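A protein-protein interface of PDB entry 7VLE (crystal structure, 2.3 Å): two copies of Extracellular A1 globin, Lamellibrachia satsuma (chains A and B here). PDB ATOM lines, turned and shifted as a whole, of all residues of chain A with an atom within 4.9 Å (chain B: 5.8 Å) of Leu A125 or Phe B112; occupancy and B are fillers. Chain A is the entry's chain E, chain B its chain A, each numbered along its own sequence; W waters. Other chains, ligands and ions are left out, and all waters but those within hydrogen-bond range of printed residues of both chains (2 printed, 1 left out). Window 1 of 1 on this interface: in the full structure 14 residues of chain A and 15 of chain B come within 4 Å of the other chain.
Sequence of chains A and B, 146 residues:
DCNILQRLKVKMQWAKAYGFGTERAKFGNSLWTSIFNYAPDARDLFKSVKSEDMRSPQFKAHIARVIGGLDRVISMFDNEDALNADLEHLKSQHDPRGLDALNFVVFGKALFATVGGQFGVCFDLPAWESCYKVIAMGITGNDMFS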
ATOM      1  N   PHE A 112      11.851  31.386 -13.656  1.00  0.00           N
ATOM      2  CA  PHE A 112      11.428  30.107 -13.092  1.00  0.00           C
ATOM      3  C   PHE A 112      12.588  29.121 -13.049  1.00  0.00           C
ATOM      4  O   PHE A 112      12.822  28.461 -12.030  1.00  0.00           O
ATOM      5  CB  PHE A 112      10.271  29.527 -13.908  1.00  0.00           C
ATOM      6  CG  PHE A 112       9.073  30.430 -14.002  1.00  0.00           C
ATOM      7  CD1 PHE A 112       8.794  31.346 -13.002  1.00  0.00           C
ATOM      8  CD2 PHE A 112       8.223  30.356 -15.094  1.00  0.00           C
ATOM      9  CE1 PHE A 112       7.692  32.174 -13.091  1.00  0.00           C
ATOM     10  CE2 PHE A 112       7.121  31.182 -15.188  1.00  0.00           C
ATOM     11  CZ  PHE A 112       6.854  32.091 -14.186  1.00  0.00           C
ATOM     12  N   PHE A 123      10.207  23.513  -5.706  1.00  0.00           N
ATOM     13  CA  PHE A 123       9.809  24.754  -6.347  1.00  0.00           C
ATOM     14  C   PHE A 123       8.379  24.645  -6.868  1.00  0.00           C
ATOM     15  O   PHE A 123       8.039  23.695  -7.579  1.00  0.00           O
ATOM     16  CB  PHE A 123      10.796  25.038  -7.479  1.00  0.00           C
ATOM     17  CG  PHE A 123      10.467  26.234  -8.312  1.00  0.00           C
ATOM     18  CD1 PHE A 123      10.657  27.509  -7.818  1.00  0.00           C
ATOM     19  CD2 PHE A 123      10.022  26.079  -9.614  1.00  0.00           C
ATOM     20  CE1 PHE A 123      10.378  28.614  -8.597  1.00  0.00           C
ATOM     21  CE2 PHE A 123       9.739  27.179 -10.399  1.00  0.00           C
ATOM     22  CZ  PHE A 123       9.916  28.449  -9.889  1.00  0.00           C
ATOM     23  N   ASP A 124       7.535  25.611  -6.505  1.00  0.00           N
ATOM     24  CA  ASP A 124       6.122  25.592  -6.888  1.00  0.00           C
ATOM     25  C   ASP A 124       5.964  26.359  -8.197  1.00  0.00           C
ATOM     26  O   ASP A 124       5.709  27.564  -8.212  1.00  0.00           O
ATOM     27  CB  ASP A 124       5.249  26.175  -5.783  1.00  0.00           C
ATOM     28  CG  ASP A 124       3.774  25.839  -5.960  1.00  0.00           C
ATOM     29  OD1 ASP A 124       3.334  25.626  -7.109  1.00  0.00           O
ATOM     30  OD2 ASP A 124       3.049  25.790  -4.944  1.00  0.00           O
ATOM     31  N   LEU A 125       6.103  25.638  -9.309  1.00  0.00           N
ATOM     32  CA  LEU A 125       5.999  26.267 -10.624  1.00  0.00           C
ATOM     33  C   LEU A 125       4.623  26.864 -10.911  1.00  0.00           C
ATOM     34  O   LEU A 125       4.573  27.975 -11.466  1.00  0.00           O
ATOM     35  CB  LEU A 125       6.392  25.256 -11.709  1.00  0.00           C
ATOM     36  CG  LEU A 125       6.385  25.751 -13.155  1.00  0.00           C
ATOM     37  CD1 LEU A 125       7.317  26.939 -13.304  1.00  0.00           C
ATOM     38  CD2 LEU A 125       6.779  24.632 -14.108  1.00  0.00           C
ATOM     39  N   PRO A 126       3.497  26.203 -10.604  1.00  0.00           N
ATOM     40  CA  PRO A 126       2.200  26.875 -10.798  1.00  0.00           C
ATOM     41  C   PRO A 126       2.072  28.173 -10.022  1.00  0.00           C
ATOM     42  O   PRO A 126       1.547  29.159 -10.555  1.00  0.00           O
ATOM     43  CB  PRO A 126       1.191  25.824 -10.315  1.00  0.00           C
ATOM     44  CG  PRO A 126       1.874  24.530 -10.540  1.00  0.00           C
ATOM     45  CD  PRO A 126       3.321  24.784 -10.242  1.00  0.00           C
ATOM     46  N   ALA A 127       2.536  28.198  -8.771  1.00  0.00           N
ATOM     47  CA  ALA A 127       2.477  29.422  -7.977  1.00  0.00           C
ATOM     48  C   ALA A 127       3.264  30.543  -8.645  1.00  0.00           C
ATOM     49  O   ALA A 127       2.781  31.676  -8.760  1.00  0.00           O
ATOM     50  CB  ALA A 127       3.011  29.158  -6.568  1.00  0.00           C
ATOM     51  N   TRP A 128       4.480  30.236  -9.101  1.00  0.00           N
ATOM     52  CA  TRP A 128       5.330  31.250  -9.715  1.00  0.00           C
ATOM     53  C   TRP A 128       4.769  31.721 -11.051  1.00  0.00           C
ATOM     54  O   TRP A 128       4.857  32.910 -11.378  1.00  0.00           O
ATOM     55  CB  TRP A 128       6.744  30.698  -9.887  1.00  0.00           C
ATOM     56  CG  TRP A 128       7.589  30.877  -8.673  1.00  0.00           C
ATOM     57  CD1 TRP A 128       7.670  30.045  -7.596  1.00  0.00           C
ATOM     58  CD2 TRP A 128       8.469  31.972  -8.404  1.00  0.00           C
ATOM     59  NE1 TRP A 128       8.557  30.551  -6.674  1.00  0.00           N
ATOM     60  CE2 TRP A 128       9.058  31.735  -7.146  1.00  0.00           C
ATOM     61  CE3 TRP A 128       8.817  33.130  -9.105  1.00  0.00           C
ATOM     62  CZ2 TRP A 128       9.978  32.613  -6.576  1.00  0.00           C
ATOM     63  CZ3 TRP A 128       9.728  34.001  -8.539  1.00  0.00           C
ATOM     64  CH2 TRP A 128      10.298  33.738  -7.286  1.00  0.00           C
ATOM     65  N   GLU A 129       4.204  30.805 -11.841  1.00  0.00           N
ATOM     66  CA  GLU A 129       3.587  31.190 -13.108  1.00  0.00           C
ATOM     67  C   GLU A 129       2.468  32.199 -12.886  1.00  0.00           C
ATOM     68  O   GLU A 129       2.393  33.225 -13.573  1.00  0.00           O
ATOM     69  CB  GLU A 129       3.045  29.953 -13.828  1.00  0.00           C
ATOM     70  CG  GLU A 129       4.089  29.104 -14.529  1.00  0.00           C
ATOM     71  CD  GLU A 129       3.491  27.856 -15.158  1.00  0.00           C
ATOM     72  OE1 GLU A 129       2.341  27.507 -14.815  1.00  0.00           O
ATOM     73  OE2 GLU A 129       4.169  27.226 -15.996  1.00  0.00           O
ATOM     74  N   TYR B  38       0.297  19.699  -6.140  1.00  0.00           N
ATOM     75  CA  TYR B  38      -0.293  20.616  -7.109  1.00  0.00           C
ATOM     76  C   TYR B  38      -1.791  20.377  -7.245  1.00  0.00           C
ATOM     77  O   TYR B  38      -2.575  21.330  -7.317  1.00  0.00           O
ATOM     78  CB  TYR B  38       0.385  20.465  -8.471  1.00  0.00           C
ATOM     79  CG  TYR B  38       1.814  20.962  -8.550  1.00  0.00           C
ATOM     80  CD1 TYR B  38       2.434  21.557  -7.458  1.00  0.00           C
ATOM     81  CD2 TYR B  38       2.537  20.844  -9.728  1.00  0.00           C
ATOM     82  CE1 TYR B  38       3.739  22.010  -7.538  1.00  0.00           C
ATOM     83  CE2 TYR B  38       3.839  21.295  -9.820  1.00  0.00           C
ATOM     84  CZ  TYR B  38       4.436  21.877  -8.723  1.00  0.00           C
ATOM     85  OH  TYR B  38       5.733  22.327  -8.814  1.00  0.00           O
ATOM     86  N   PHE B 107       0.888  17.160 -14.489  1.00  0.00           N
ATOM     87  CA  PHE B 107       2.058  16.291 -14.568  1.00  0.00           C
ATOM     88  C   PHE B 107       3.253  17.032 -15.151  1.00  0.00           C
ATOM     89  O   PHE B 107       4.382  16.891 -14.663  1.00  0.00           O
ATOM     90  CB  PHE B 107       1.726  15.058 -15.414  1.00  0.00           C
ATOM     91  CG  PHE B 107       2.842  14.048 -15.507  1.00  0.00           C
ATOM     92  CD1 PHE B 107       3.913  14.241 -16.370  1.00  0.00           C
ATOM     93  CD2 PHE B 107       2.802  12.886 -14.755  1.00  0.00           C
ATOM     94  CE1 PHE B 107       4.932  13.312 -16.457  1.00  0.00           C
ATOM     95  CE2 PHE B 107       3.817  11.949 -14.842  1.00  0.00           C
ATOM     96  CZ  PHE B 107       4.881  12.162 -15.695  1.00  0.00           C
ATOM     97  N   GLY B 108       3.021  17.822 -16.201  1.00  0.00           N
ATOM     98  CA  GLY B 108       4.117  18.540 -16.831  1.00  0.00           C
ATOM     99  C   GLY B 108       4.762  19.550 -15.904  1.00  0.00           C
ATOM    100  O   GLY B 108       5.989  19.629 -15.812  1.00  0.00           O
ATOM    101  N   LYS B 109       3.940  20.337 -15.205  1.00  0.00           N
ATOM    102  CA  LYS B 109       4.463  21.302 -14.240  1.00  0.00           C
ATOM    103  C   LYS B 109       5.322  20.616 -13.188  1.00  0.00           C
ATOM    104  O   LYS B 109       6.416  21.085 -12.854  1.00  0.00           O
ATOM    105  CB  LYS B 109       3.310  22.055 -13.570  1.00  0.00           C
ATOM    106  CG  LYS B 109       2.922  23.367 -14.231  1.00  0.00           C
ATOM    107  CD  LYS B 109       2.351  23.154 -15.619  1.00  0.00           C
ATOM    108  CE  LYS B 109       1.997  24.479 -16.274  1.00  0.00           C
ATOM    109  NZ  LYS B 109       0.957  25.217 -15.509  1.00  0.00           N
ATOM    110  N   ALA B 110       4.832  19.497 -12.647  1.00  0.00           N
ATOM    111  CA  ALA B 110       5.579  18.765 -11.632  1.00  0.00           C
ATOM    112  C   ALA B 110       6.867  18.180 -12.195  1.00  0.00           C
ATOM    113  O   ALA B 110       7.871  18.093 -11.481  1.00  0.00           O
ATOM    114  CB  ALA B 110       4.708  17.660 -11.042  1.00  0.00           C
ATOM    115  N   LEU B 111       6.851  17.774 -13.465  1.00  0.00           N
ATOM    116  CA  LEU B 111       8.052  17.246 -14.101  1.00  0.00           C
ATOM    117  C   LEU B 111       9.100  18.335 -14.292  1.00  0.00           C
ATOM    118  O   LEU B 111      10.289  18.115 -14.030  1.00  0.00           O
ATOM    119  CB  LEU B 111       7.685  16.610 -15.441  1.00  0.00           C
ATOM    120  CG  LEU B 111       8.831  16.130 -16.328  1.00  0.00           C
ATOM    121  CD1 LEU B 111       9.562  14.967 -15.674  1.00  0.00           C
ATOM    122  CD2 LEU B 111       8.314  15.745 -17.706  1.00  0.00           C
ATOM    123  N   PHE B 112       8.676  19.518 -14.747  1.00  0.00           N
ATOM    124  CA  PHE B 112       9.601  20.630 -14.938  1.00  0.00           C
ATOM    125  C   PHE B 112      10.254  21.029 -13.623  1.00  0.00           C
ATOM    126  O   PHE B 112      11.469  21.252 -13.557  1.00  0.00           O
ATOM    127  CB  PHE B 112       8.867  21.834 -15.538  1.00  0.00           C
ATOM    128  CG  PHE B 112       8.101  21.529 -16.792  1.00  0.00           C
ATOM    129  CD1 PHE B 112       8.504  20.516 -17.648  1.00  0.00           C
ATOM    130  CD2 PHE B 112       6.974  22.267 -17.118  1.00  0.00           C
ATOM    131  CE1 PHE B 112       7.793  20.243 -18.802  1.00  0.00           C
ATOM    132  CE2 PHE B 112       6.260  21.999 -18.269  1.00  0.00           C
ATOM    133  CZ  PHE B 112       6.671  20.985 -19.113  1.00  0.00           C
ATOM    134  N   ALA B 113       9.450  21.137 -12.562  1.00  0.00           N
ATOM    135  CA  ALA B 113       9.977  21.536 -11.262  1.00  0.00           C
ATOM    136  C   ALA B 113      10.963  20.507 -10.727  1.00  0.00           C
ATOM    137  O   ALA B 113      12.002  20.867 -10.161  1.00  0.00           O
ATOM    138  CB  ALA B 113       8.828  21.739 -10.275  1.00  0.00           C
ATOM    139  N   THR B 114      10.658  19.219 -10.905  1.00  0.00           N
ATOM    140  CA  THR B 114      11.520  18.166 -10.379  1.00  0.00           C
ATOM    141  C   THR B 114      12.833  18.088 -11.150  1.00  0.00           C
ATOM    142  O   THR B 114      13.912  18.025 -10.549  1.00  0.00           O
ATOM    143  CB  THR B 114      10.792  16.821 -10.426  1.00  0.00           C
ATOM    144  OG1 THR B 114       9.535  16.927  -9.744  1.00  0.00           O
ATOM    145  CG2 THR B 114      11.628  15.743  -9.758  1.00  0.00           C
ATOM    146  N   VAL B 115      12.761  18.077 -12.484  1.00  0.00           N
ATOM    147  CA  VAL B 115      13.976  18.016 -13.294  1.00  0.00           C
ATOM    148  C   VAL B 115      14.819  19.266 -13.079  1.00  0.00           C
ATOM    149  O   VAL B 115      16.029  19.190 -12.843  1.00  0.00           O
ATOM    150  CB  VAL B 115      13.631  17.836 -14.784  1.00  0.00           C
ATOM    151  CG1 VAL B 115      14.892  17.950 -15.631  1.00  0.00           C
ATOM    152  CG2 VAL B 115      12.952  16.504 -15.024  1.00  0.00           C
ATOM    153  N   GLY B 116      14.186  20.438 -13.168  1.00  0.00           N
ATOM    154  CA  GLY B 116      14.926  21.680 -13.025  1.00  0.00           C
ATOM    155  C   GLY B 116      15.506  21.858 -11.636  1.00  0.00           C
ATOM    156  O   GLY B 116      16.630  22.344 -11.481  1.00  0.00           O
ATOM    157  N   GLY B 117      14.750  21.471 -10.606  1.00  0.00           N
ATOM    158  CA  GLY B 117      15.264  21.529  -9.251  1.00  0.00           C
ATOM    159  C   GLY B 117      16.385  20.551  -8.983  1.00  0.00           C
ATOM    160  O   GLY B 117      17.146  20.740  -8.029  1.00  0.00           O
ATOM    161  N   PHE B 123      18.630  24.605 -16.506  1.00  0.00           N
ATOM    162  CA  PHE B 123      17.424  23.953 -16.992  1.00  0.00           C
ATOM    163  C   PHE B 123      16.774  24.780 -18.097  1.00  0.00           C
ATOM    164  O   PHE B 123      16.509  25.972 -17.923  1.00  0.00           O
ATOM    165  CB  PHE B 123      16.464  23.765 -15.817  1.00  0.00           C
ATOM    166  CG  PHE B 123      15.175  23.093 -16.175  1.00  0.00           C
ATOM    167  CD1 PHE B 123      15.155  21.760 -16.545  1.00  0.00           C
ATOM    168  CD2 PHE B 123      13.977  23.785 -16.104  1.00  0.00           C
ATOM    169  CE1 PHE B 123      13.966  21.133 -16.862  1.00  0.00           C
ATOM    170  CE2 PHE B 123      12.784  23.164 -16.420  1.00  0.00           C
ATOM    171  CZ  PHE B 123      12.778  21.836 -16.800  1.00  0.00           C
ATOM    172  N   LEU B 125      13.717  25.455 -19.572  1.00  0.00           N
ATOM    173  CA  LEU B 125      12.273  25.321 -19.388  1.00  0.00           C
ATOM    174  C   LEU B 125      11.477  25.425 -20.689  1.00  0.00           C
ATOM    175  O   LEU B 125      10.560  24.612 -20.885  1.00  0.00           O
ATOM    176  CB  LEU B 125      11.790  26.350 -18.359  1.00  0.00           C
ATOM    177  CG  LEU B 125      10.280  26.444 -18.126  1.00  0.00           C
ATOM    178  CD1 LEU B 125       9.715  25.099 -17.697  1.00  0.00           C
ATOM    179  CD2 LEU B 125       9.960  27.515 -17.095  1.00  0.00           C
ATOM    180  N   TRP B 128      11.589  22.120 -22.475  1.00  0.00           N
ATOM    181  CA  TRP B 128      10.827  21.086 -21.785  1.00  0.00           C
ATOM    182  C   TRP B 128       9.326  21.310 -21.923  1.00  0.00           C
ATOM    183  O   TRP B 128       8.563  20.340 -21.990  1.00  0.00           O
ATOM    184  CB  TRP B 128      11.232  21.035 -20.312  1.00  0.00           C
ATOM    185  CG  TRP B 128      12.503  20.281 -20.078  1.00  0.00           C
ATOM    186  CD1 TRP B 128      13.776  20.765 -20.166  1.00  0.00           C
ATOM    187  CD2 TRP B 128      12.623  18.900 -19.721  1.00  0.00           C
ATOM    188  NE1 TRP B 128      14.682  19.770 -19.882  1.00  0.00           N
ATOM    189  CE2 TRP B 128      13.999  18.616 -19.606  1.00  0.00           C
ATOM    190  CE3 TRP B 128      11.701  17.876 -19.487  1.00  0.00           C
ATOM    191  CZ2 TRP B 128      14.472  17.351 -19.269  1.00  0.00           C
ATOM    192  CZ3 TRP B 128      12.172  16.623 -19.151  1.00  0.00           C
ATOM    193  CH2 TRP B 128      13.546  16.370 -19.044  1.00  0.00           C
ATOM    194  N   GLU B 129       8.887  22.570 -21.965  1.00  0.00           N
ATOM    195  CA  GLU B 129       7.481  22.854 -22.226  1.00  0.00           C
ATOM    196  C   GLU B 129       7.080  22.395 -23.623  1.00  0.00           C
ATOM    197  O   GLU B 129       6.016  21.793 -23.806  1.00  0.00           O
ATOM    198  CB  GLU B 129       7.206  24.350 -22.059  1.00  0.00           C
ATOM    199  CG  GLU B 129       7.296  24.855 -20.628  1.00  0.00           C
ATOM    200  CD  GLU B 129       7.009  26.342 -20.519  1.00  0.00           C
ATOM    201  OE1 GLU B 129       7.295  27.076 -21.489  1.00  0.00           O
ATOM    202  OE2 GLU B 129       6.491  26.775 -19.469  1.00  0.00           O
ATOM    203  N   TYR B 132       7.459  18.355 -23.875  1.00  0.00           N
ATOM    204  CA  TYR B 132       6.451  17.630 -23.110  1.00  0.00           C
ATOM    205  C   TYR B 132       5.104  17.677 -23.813  1.00  0.00           C
ATOM    206  O   TYR B 132       4.339  16.706 -23.764  1.00  0.00           O
ATOM    207  CB  TYR B 132       6.323  18.185 -21.693  1.00  0.00           C
ATOM    208  CG  TYR B 132       5.213  17.508 -20.921  1.00  0.00           C
ATOM    209  CD1 TYR B 132       3.980  18.126 -20.744  1.00  0.00           C
ATOM    210  CD2 TYR B 132       5.386  16.234 -20.399  1.00  0.00           C
ATOM    211  CE1 TYR B 132       2.959  17.499 -20.050  1.00  0.00           C
ATOM    212  CE2 TYR B 132       4.373  15.600 -19.705  1.00  0.00           C
ATOM    213  CZ  TYR B 132       3.162  16.235 -19.532  1.00  0.00           C
ATOM    214  OH  TYR B 132       2.153  15.604 -18.840  1.00  0.00           O
HETATM  215  O   HOH W   1       5.062  25.351 -17.519  1.00  0.00           O
HETATM  216  O   HOH W   2       6.940  21.292  -6.699  1.00  0.00           O
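The side-chain hydroxyl of Tyr B38 lies within hydrogen-bond range of the backbone carbonyl oxygen of Phe A123. The side-chain hydroxyl of Tyr B38 is in hydrogen-bond range of the backbone NH of Leu A125 (3.4 Å). The side-chain amino group (NZ) of Lys B109 lies within salt-bridge range of the side-chain carboxylate (OE1) of Glu A129, 2.8 Å away.
N of Ala A127 is in hydrogen-bond range of OD1 of Asp A124, at 3.2 Å.
Phe A112 touches Leu B125 (CB to CD2, 3.8 Å). Ala B113 touches Phe A123. Asp A124 touches Tyr B38. Lys B109 touches Leu A125. Phe B112 touches Leu A125 (CB to CD2, 3.8 Å). Tyr B38 touches Pro A126.
Of the printed residues of chain B, Phe A112 touches Leu B125 (3.8 Å). Of chain B, only Tyr B38 (3.4 Å), Lys B109 (3.8 Å) and Phe B112 (3.8 Å) come within 4 Å of Leu A125. Printed residues of chain B within 4 Å of Pro A126: Tyr B38 (3.5 Å). Of the printed residues of chain A, Tyr B38 touches Phe A123, Asp A124, Leu A125 and Pro A126. Of chain A, only Leu A125 comes within 4 Å of Phe B112. Thr B114 touches none of the printed residues of chain A. Of the printed residues of chain A, Leu B125 touches Phe A112 (3.8 Å). The nearest residue of chain B that does not touch Leu A125 is Ala B113 (4.5 Å).
Along chain B the printed residues that touch a printed residue of chain A span positions 38 to 125. Printed residues of chain A that touch a printed residue of chain B: Phe A112, Phe A123, Asp A124, Leu A125, Pro A126 and Glu A129. Among the printed residues, 9 pairs touch across the chains.
Phe A112 touches Leu B125, and with the chains exchanged Leu A125 touches Phe B112. Of the 9 pairs that touch across the chains among the printed residues, 2 have their exchanged pair printed and touching as well.
Water W1 bridges OE2 of Glu A129 (2.6 Å) and OE2 of Glu B129 (2.8 Å). Water W2 lies within hydrogen-bond range of the side-chain hydroxyl (OH) of Tyr B38 (2.6 Å) and the backbone carbonyl oxygen (O) of Phe A123 (2.8 Å).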
